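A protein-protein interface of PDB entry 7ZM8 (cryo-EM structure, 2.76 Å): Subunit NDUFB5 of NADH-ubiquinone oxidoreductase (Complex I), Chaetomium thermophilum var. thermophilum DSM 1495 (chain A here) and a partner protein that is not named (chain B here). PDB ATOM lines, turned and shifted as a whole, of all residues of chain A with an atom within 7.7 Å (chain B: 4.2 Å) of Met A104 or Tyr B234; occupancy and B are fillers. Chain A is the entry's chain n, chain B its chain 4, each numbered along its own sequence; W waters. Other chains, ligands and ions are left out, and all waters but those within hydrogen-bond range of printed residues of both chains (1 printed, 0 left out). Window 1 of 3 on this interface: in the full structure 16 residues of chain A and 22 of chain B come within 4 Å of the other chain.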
ATOM      1  N   GLU A  98       3.241 -19.535 -25.091  1.00  0.00           N
ATOM      2  CA  GLU A  98       1.998 -20.241 -24.805  1.00  0.00           C
ATOM      3  C   GLU A  98       1.584 -20.101 -23.347  1.00  0.00           C
ATOM      4  O   GLU A  98       0.401 -19.892 -23.056  1.00  0.00           O
ATOM      5  CB  GLU A  98       2.127 -21.712 -25.183  1.00  0.00           C
ATOM      6  CG  GLU A  98       0.811 -22.437 -25.117  1.00  0.00           C
ATOM      7  CD  GLU A  98       0.498 -22.895 -23.705  1.00  0.00           C
ATOM      8  OE1 GLU A  98       1.448 -23.157 -22.937  1.00  0.00           O
ATOM      9  OE2 GLU A  98      -0.690 -22.904 -23.330  1.00  0.00           O
ATOM     10  N   THR A  99       2.528 -20.234 -22.417  1.00  0.00           N
ATOM     11  CA  THR A  99       2.151 -20.205 -21.010  1.00  0.00           C
ATOM     12  C   THR A  99       1.669 -18.824 -20.592  1.00  0.00           C
ATOM     13  O   THR A  99       0.822 -18.709 -19.704  1.00  0.00           O
ATOM     14  CB  THR A  99       3.319 -20.661 -20.133  1.00  0.00           C
ATOM     15  OG1 THR A  99       2.905 -20.692 -18.761  1.00  0.00           O
ATOM     16  CG2 THR A  99       4.495 -19.723 -20.265  1.00  0.00           C
ATOM     17  N   ARG A 100       2.101 -17.784 -21.282  1.00  0.00           N
ATOM     18  CA  ARG A 100       1.734 -16.419 -20.843  1.00  0.00           C
ATOM     19  C   ARG A 100       0.438 -16.024 -21.527  1.00  0.00           C
ATOM     20  O   ARG A 100      -0.359 -15.336 -20.896  1.00  0.00           O
ATOM     21  CB  ARG A 100       2.872 -15.454 -21.176  1.00  0.00           C
ATOM     22  CG  ARG A 100       4.111 -15.617 -20.309  1.00  0.00           C
ATOM     23  CD  ARG A 100       5.215 -14.706 -20.801  1.00  0.00           C
ATOM     24  NE  ARG A 100       6.462 -14.924 -20.085  1.00  0.00           N
ATOM     25  CZ  ARG A 100       6.814 -14.284 -18.978  1.00  0.00           C
ATOM     26  NH1 ARG A 100       6.009 -13.376 -18.454  1.00  0.00           N
ATOM     27  NH2 ARG A 100       7.970 -14.551 -18.398  1.00  0.00           N
ATOM     28  N   ASN A 101       0.248 -16.464 -22.759  1.00  0.00           N
ATOM     29  CA  ASN A 101      -0.995 -16.182 -23.518  1.00  0.00           C
ATOM     30  C   ASN A 101      -2.159 -16.894 -22.867  1.00  0.00           C
ATOM     31  O   ASN A 101      -3.231 -16.305 -22.805  1.00  0.00           O
ATOM     32  CB  ASN A 101      -0.894 -16.635 -24.975  1.00  0.00           C
ATOM     33  CG  ASN A 101      -0.230 -15.622 -25.881  1.00  0.00           C
ATOM     34  OD1 ASN A 101      -0.751 -14.535 -26.097  1.00  0.00           O
ATOM     35  ND2 ASN A 101       0.914 -15.975 -26.434  1.00  0.00           N
ATOM     36  N   THR A 102      -1.945 -18.132 -22.445  1.00  0.00           N
ATOM     37  CA  THR A 102      -3.017 -18.948 -21.830  1.00  0.00           C
ATOM     38  C   THR A 102      -3.468 -18.332 -20.514  1.00  0.00           C
ATOM     39  O   THR A 102      -4.678 -18.295 -20.278  1.00  0.00           O
ATOM     40  CB  THR A 102      -2.571 -20.408 -21.718  1.00  0.00           C
ATOM     41  OG1 THR A 102      -2.086 -20.755 -23.011  1.00  0.00           O
ATOM     42  CG2 THR A 102      -3.692 -21.343 -21.325  1.00  0.00           C
ATOM     43  N   LEU A 103      -2.528 -17.858 -19.707  1.00  0.00           N
ATOM     44  CA  LEU A 103      -2.896 -17.183 -18.446  1.00  0.00           C
ATOM     45  C   LEU A 103      -3.701 -15.926 -18.762  1.00  0.00           C
ATOM     46  O   LEU A 103      -4.727 -15.717 -18.111  1.00  0.00           O
ATOM     47  CB  LEU A 103      -1.621 -16.867 -17.667  1.00  0.00           C
ATOM     48  CG  LEU A 103      -0.947 -18.058 -16.994  1.00  0.00           C
ATOM     49  CD1 LEU A 103       0.353 -17.636 -16.332  1.00  0.00           C
ATOM     50  CD2 LEU A 103      -1.879 -18.703 -15.981  1.00  0.00           C
ATOM     51  N   MET A 104      -3.273 -15.132 -19.737  1.00  0.00           N
ATOM     52  CA  MET A 104      -3.966 -13.877 -19.990  1.00  0.00           C
ATOM     53  C   MET A 104      -5.340 -14.119 -20.593  1.00  0.00           C
ATOM     54  O   MET A 104      -6.305 -13.427 -20.252  1.00  0.00           O
ATOM     55  CB  MET A 104      -3.118 -12.990 -20.904  1.00  0.00           C
ATOM     56  CG  MET A 104      -3.514 -11.524 -20.907  1.00  0.00           C
ATOM     57  SD  MET A 104      -3.422 -10.605 -19.350  1.00  0.00           S
ATOM     58  CE  MET A 104      -2.211 -11.518 -18.392  1.00  0.00           C
ATOM     59  N   ALA A 105      -5.447 -15.092 -21.495  1.00  0.00           N
ATOM     60  CA  ALA A 105      -6.743 -15.436 -22.063  1.00  0.00           C
ATOM     61  C   ALA A 105      -7.701 -15.929 -20.986  1.00  0.00           C
ATOM     62  O   ALA A 105      -8.897 -15.625 -21.024  1.00  0.00           O
ATOM     63  CB  ALA A 105      -6.567 -16.487 -23.156  1.00  0.00           C
ATOM     64  N   ALA A 106      -7.194 -16.693 -20.021  1.00  0.00           N
ATOM     65  CA  ALA A 106      -8.036 -17.198 -18.945  1.00  0.00           C
ATOM     66  C   ALA A 106      -8.608 -16.067 -18.100  1.00  0.00           C
ATOM     67  O   ALA A 106      -9.794 -16.081 -17.754  1.00  0.00           O
ATOM     68  CB  ALA A 106      -7.237 -18.166 -18.076  1.00  0.00           C
ATOM     69  N   ALA A 107      -7.829 -15.040 -17.782  1.00  0.00           N
ATOM     70  CA  ALA A 107      -8.278 -13.924 -16.922  1.00  0.00           C
ATOM     71  C   ALA A 107      -9.268 -13.037 -17.663  1.00  0.00           C
ATOM     72  O   ALA A 107     -10.294 -12.681 -17.086  1.00  0.00           O
ATOM     73  CB  ALA A 107      -7.084 -13.131 -16.501  1.00  0.00           C
ATOM     74  N   LEU A 108      -8.938 -12.662 -18.895  1.00  0.00           N
ATOM     75  CA  LEU A 108      -9.815 -11.761 -19.682  1.00  0.00           C
ATOM     76  C   LEU A 108     -11.115 -12.494 -19.994  1.00  0.00           C
ATOM     77  O   LEU A 108     -12.129 -11.806 -20.191  1.00  0.00           O
ATOM     78  CB  LEU A 108      -9.055 -11.274 -20.915  1.00  0.00           C
ATOM     79  CG  LEU A 108      -8.118 -10.105 -20.622  1.00  0.00           C
ATOM     80  CD1 LEU A 108      -6.860 -10.165 -21.465  1.00  0.00           C
ATOM     81  CD2 LEU A 108      -8.835  -8.780 -20.802  1.00  0.00           C
ATOM     82  N   GLU A 109     -11.088 -13.826 -20.032  1.00  0.00           N
ATOM     83  CA  GLU A 109     -12.343 -14.602 -20.162  1.00  0.00           C
ATOM     84  C   GLU A 109     -13.125 -14.519 -18.852  1.00  0.00           C
ATOM     85  O   GLU A 109     -14.365 -14.431 -18.924  1.00  0.00           O
ATOM     86  CB  GLU A 109     -12.021 -16.066 -20.411  1.00  0.00           C
ATOM     87  CG  GLU A 109     -11.698 -16.395 -21.854  1.00  0.00           C
ATOM     88  CD  GLU A 109     -12.913 -16.575 -22.745  1.00  0.00           C
ATOM     89  OE1 GLU A 109     -14.041 -16.539 -22.218  1.00  0.00           O
ATOM     90  OE2 GLU A 109     -12.727 -16.749 -23.964  1.00  0.00           O
ATOM     91  N   GLN A 110     -12.456 -14.557 -17.704  1.00  0.00           N
ATOM     92  CA  GLN A 110     -13.150 -14.447 -16.399  1.00  0.00           C
ATOM     93  C   GLN A 110     -13.806 -13.073 -16.294  1.00  0.00           C
ATOM     94  O   GLN A 110     -14.964 -13.007 -15.881  1.00  0.00           O
ATOM     95  CB  GLN A 110     -12.201 -14.691 -15.232  1.00  0.00           C
ATOM     96  CG  GLN A 110     -12.875 -14.626 -13.870  1.00  0.00           C
ATOM     97  CD  GLN A 110     -13.910 -15.707 -13.682  1.00  0.00           C
ATOM     98  OE1 GLN A 110     -14.998 -15.469 -13.164  1.00  0.00           O
ATOM     99  NE2 GLN A 110     -13.578 -16.914 -14.111  1.00  0.00           N
ATOM    100  N   ASN B 110       0.452  -9.198 -18.111  1.00  0.00           N
ATOM    101  CA  ASN B 110      -0.166  -8.069 -17.369  1.00  0.00           C
ATOM    102  C   ASN B 110      -0.473  -8.541 -15.946  1.00  0.00           C
ATOM    103  O   ASN B 110       0.168  -7.999 -15.020  1.00  0.00           O
ATOM    104  CB  ASN B 110      -1.397  -7.518 -18.085  1.00  0.00           C
ATOM    105  CG  ASN B 110      -1.800  -6.145 -17.590  1.00  0.00           C
ATOM    106  OD1 ASN B 110      -1.080  -5.523 -16.811  1.00  0.00           O
ATOM    107  ND2 ASN B 110      -2.944  -5.660 -18.039  1.00  0.00           N
ATOM    108  N   LEU B 111      -1.466  -9.422 -15.773  1.00  0.00           N
ATOM    109  CA  LEU B 111      -1.795 -10.022 -14.445  1.00  0.00           C
ATOM    110  C   LEU B 111      -2.551  -8.999 -13.593  1.00  0.00           C
ATOM    111  O   LEU B 111      -2.903  -9.329 -12.445  1.00  0.00           O
ATOM    112  CB  LEU B 111      -0.532 -10.554 -13.755  1.00  0.00           C
ATOM    113  CG  LEU B 111      -0.740 -11.739 -12.813  1.00  0.00           C
ATOM    114  CD1 LEU B 111      -1.489 -12.862 -13.513  1.00  0.00           C
ATOM    115  CD2 LEU B 111       0.588 -12.239 -12.268  1.00  0.00           C
ATOM    116  N   TYR B 119      -2.350  -4.072 -24.229  1.00  0.00           N
ATOM    117  CA  TYR B 119      -1.837  -5.451 -24.390  1.00  0.00           C
ATOM    118  C   TYR B 119      -1.088  -5.526 -25.725  1.00  0.00           C
ATOM    119  O   TYR B 119      -1.751  -5.379 -26.756  1.00  0.00           O
ATOM    120  CB  TYR B 119      -2.991  -6.454 -24.404  1.00  0.00           C
ATOM    121  CG  TYR B 119      -3.828  -6.500 -23.151  1.00  0.00           C
ATOM    122  CD1 TYR B 119      -3.313  -6.991 -21.964  1.00  0.00           C
ATOM    123  CD2 TYR B 119      -5.144  -6.073 -23.159  1.00  0.00           C
ATOM    124  CE1 TYR B 119      -4.082  -7.044 -20.814  1.00  0.00           C
ATOM    125  CE2 TYR B 119      -5.926  -6.119 -22.019  1.00  0.00           C
ATOM    126  CZ  TYR B 119      -5.393  -6.605 -20.840  1.00  0.00           C
ATOM    127  OH  TYR B 119      -6.156  -6.651 -19.711  1.00  0.00           O
ATOM    128  N   LEU B 173      -3.695  -5.812 -28.862  1.00  0.00           N
ATOM    129  CA  LEU B 173      -4.363  -7.136 -28.961  1.00  0.00           C
ATOM    130  C   LEU B 173      -5.829  -7.025 -28.549  1.00  0.00           C
ATOM    131  O   LEU B 173      -6.377  -8.039 -28.130  1.00  0.00           O
ATOM    132  CB  LEU B 173      -3.618  -8.125 -28.067  1.00  0.00           C
ATOM    133  CG  LEU B 173      -2.163  -8.415 -28.418  1.00  0.00           C
ATOM    134  CD1 LEU B 173      -1.615  -9.488 -27.496  1.00  0.00           C
ATOM    135  CD2 LEU B 173      -2.042  -8.849 -29.862  1.00  0.00           C
ATOM    136  N   ASP B 174      -6.423  -5.828 -28.634  1.00  0.00           N
ATOM    137  CA  ASP B 174      -7.872  -5.633 -28.360  1.00  0.00           C
ATOM    138  C   ASP B 174      -8.442  -4.827 -29.521  1.00  0.00           C
ATOM    139  O   ASP B 174      -7.649  -4.179 -30.217  1.00  0.00           O
ATOM    140  CB  ASP B 174      -8.149  -4.808 -27.105  1.00  0.00           C
ATOM    141  CG  ASP B 174      -7.739  -5.450 -25.794  1.00  0.00           C
ATOM    142  OD1 ASP B 174      -7.035  -6.469 -25.826  1.00  0.00           O
ATOM    143  OD2 ASP B 174      -8.129  -4.913 -24.747  1.00  0.00           O
ATOM    144  N   THR B 232     -15.616  -8.673 -23.681  1.00  0.00           N
ATOM    145  CA  THR B 232     -14.252  -8.126 -23.826  1.00  0.00           C
ATOM    146  C   THR B 232     -13.940  -8.046 -25.313  1.00  0.00           C
ATOM    147  O   THR B 232     -14.709  -8.612 -26.094  1.00  0.00           O
ATOM    148  CB  THR B 232     -13.202  -9.022 -23.146  1.00  0.00           C
ATOM    149  OG1 THR B 232     -11.895  -8.504 -23.385  1.00  0.00           O
ATOM    150  CG2 THR B 232     -13.253 -10.460 -23.608  1.00  0.00           C
ATOM    151  N   THR B 233     -12.932  -7.255 -25.672  1.00  0.00           N
ATOM    152  CA  THR B 233     -12.499  -7.122 -27.087  1.00  0.00           C
ATOM    153  C   THR B 233     -11.101  -7.709 -27.264  1.00  0.00           C
ATOM    154  O   THR B 233     -10.548  -7.505 -28.348  1.00  0.00           O
ATOM    155  CB  THR B 233     -12.622  -5.665 -27.545  1.00  0.00           C
ATOM    156  OG1 THR B 233     -11.979  -4.818 -26.594  1.00  0.00           O
ATOM    157  CG2 THR B 233     -14.059  -5.231 -27.710  1.00  0.00           C
ATOM    158  N   TYR B 234     -10.558  -8.356 -26.229  1.00  0.00           N
ATOM    159  CA  TYR B 234      -9.245  -9.038 -26.341  1.00  0.00           C
ATOM    160  C   TYR B 234      -9.362 -10.053 -27.475  1.00  0.00           C
ATOM    161  O   TYR B 234     -10.322 -10.827 -27.456  1.00  0.00           O
ATOM    162  CB  TYR B 234      -8.871  -9.649 -24.991  1.00  0.00           C
ATOM    163  CG  TYR B 234      -7.544 -10.360 -24.929  1.00  0.00           C
ATOM    164  CD1 TYR B 234      -6.352  -9.659 -24.990  1.00  0.00           C
ATOM    165  CD2 TYR B 234      -7.483 -11.733 -24.767  1.00  0.00           C
ATOM    166  CE1 TYR B 234      -5.129 -10.307 -24.914  1.00  0.00           C
ATOM    167  CE2 TYR B 234      -6.271 -12.395 -24.683  1.00  0.00           C
ATOM    168  CZ  TYR B 234      -5.090 -11.681 -24.760  1.00  0.00           C
ATOM    169  OH  TYR B 234      -3.897 -12.338 -24.685  1.00  0.00           O
ATOM    170  N   PHE B 235      -8.389 -10.099 -28.383  1.00  0.00           N
ATOM    171  CA  PHE B 235      -8.535 -10.942 -29.598  1.00  0.00           C
ATOM    172  C   PHE B 235      -8.742 -12.418 -29.254  1.00  0.00           C
ATOM    173  O   PHE B 235      -9.656 -13.014 -29.825  1.00  0.00           O
ATOM    174  CB  PHE B 235      -7.293 -10.823 -30.486  1.00  0.00           C
ATOM    175  CG  PHE B 235      -7.071  -9.503 -31.179  1.00  0.00           C
ATOM    176  CD1 PHE B 235      -8.117  -8.629 -31.419  1.00  0.00           C
ATOM    177  CD2 PHE B 235      -5.808  -9.150 -31.623  1.00  0.00           C
ATOM    178  CE1 PHE B 235      -7.897  -7.423 -32.066  1.00  0.00           C
ATOM    179  CE2 PHE B 235      -5.590  -7.944 -32.269  1.00  0.00           C
ATOM    180  CZ  PHE B 235      -6.635  -7.080 -32.487  1.00  0.00           C
ATOM    181  N   ASP B 236      -7.968 -12.978 -28.327  1.00  0.00           N
ATOM    182  CA  ASP B 236      -8.071 -14.438 -28.060  1.00  0.00           C
ATOM    183  C   ASP B 236      -9.514 -14.819 -27.713  1.00  0.00           C
ATOM    184  O   ASP B 236      -9.971 -15.849 -28.216  1.00  0.00           O
ATOM    185  CB  ASP B 236      -7.058 -14.891 -27.013  1.00  0.00           C
ATOM    186  CG  ASP B 236      -5.627 -14.910 -27.521  1.00  0.00           C
ATOM    187  OD1 ASP B 236      -5.448 -14.968 -28.753  1.00  0.00           O
ATOM    188  OD2 ASP B 236      -4.705 -14.866 -26.681  1.00  0.00           O
ATOM    189  N   VAL B 237     -10.207 -14.007 -26.918  1.00  0.00           N
ATOM    190  CA  VAL B 237     -11.589 -14.318 -26.463  1.00  0.00           C
ATOM    191  C   VAL B 237     -12.585 -13.988 -27.578  1.00  0.00           C
ATOM    192  O   VAL B 237     -13.547 -14.735 -27.722  1.00  0.00           O
ATOM    193  CB  VAL B 237     -11.886 -13.578 -25.144  1.00  0.00           C
ATOM    194  CG1 VAL B 237     -13.227 -13.971 -24.552  1.00  0.00           C
ATOM    195  CG2 VAL B 237     -10.772 -13.770 -24.132  1.00  0.00           C
ATOM    196  N   LEU B 238     -12.342 -12.924 -28.351  1.00  0.00           N
ATOM    197  CA  LEU B 238     -13.287 -12.551 -29.398  1.00  0.00           C
ATOM    198  C   LEU B 238     -13.240 -13.530 -30.565  1.00  0.00           C
ATOM    199  O   LEU B 238     -14.270 -13.821 -31.180  1.00  0.00           O
ATOM    200  CB  LEU B 238     -12.995 -11.126 -29.866  1.00  0.00           C
ATOM    201  CG  LEU B 238     -13.897 -10.413 -30.877  1.00  0.00           C
ATOM    202  CD1 LEU B 238     -15.359 -10.411 -30.461  1.00  0.00           C
ATOM    203  CD2 LEU B 238     -13.401  -8.997 -31.081  1.00  0.00           C
HETATM  204  O   HOH W   1      -2.264 -16.385 -28.437  1.00  0.00           O
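OG1 of Thr B232 sits at hydrogen-bond distance from N of Tyr B234 (3.1 Å). OH of Tyr B234 is in hydrogen-bond range of OD2 of Asp B236. The backbone NH of Leu B173 sits at hydrogen-bond distance from the backbone carbonyl oxygen of Tyr B119, at 2.9 Å.
Among the printed residues, merely in contact across the chains: Met A104 with Asn B110, Met A104 with Leu B111, Met A104 with Tyr B119, Met A104 with Tyr B234, Leu A108 with Tyr B119, Leu A108 with Thr B232, Leu A108 with Tyr B234 and Glu A109 with Val B237.
Water W1 lies within hydrogen-bond range of the side-chain amide oxygen (OD1) of Asn A101 and the side-chain carboxylate (OD2) of Asp B236.
Of the printed residues of chain A, Leu B111 touches Met A104. Of the printed residues of chain A, Tyr B119 touches Met A104 and Leu A108. Printed residues of chain A within 4 Å of Tyr B234: Met A104 and Leu A108. The nearest residue of chain A that does not touch Tyr B234 is Ala A105 (4.04 Å). The nearest printed residue of chain A that does not touch Leu B111 is Leu A103 (5.8 Å).
Of the 13 printed residues of chain A, 3 touch a printed residue of chain B. Printed residues of chain A that touch a printed residue of chain B: Met A104, Leu A108 and Glu A109. Hydrophobic or aromatic side chains of chain A within 4 Å of the printed part of chain B: Met A104 and Leu A108. Hydrophobic or aromatic side chains of chain B within 4 Å of the printed part of chain A: Tyr B119, Tyr B234 and Val B237. Among the printed residues, 8 pairs touch across the chains. Among the printed residues, no Asp or Glu carboxylate lies within 4 Å of a Lys or Arg side-chain nitrogen of the other chain.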
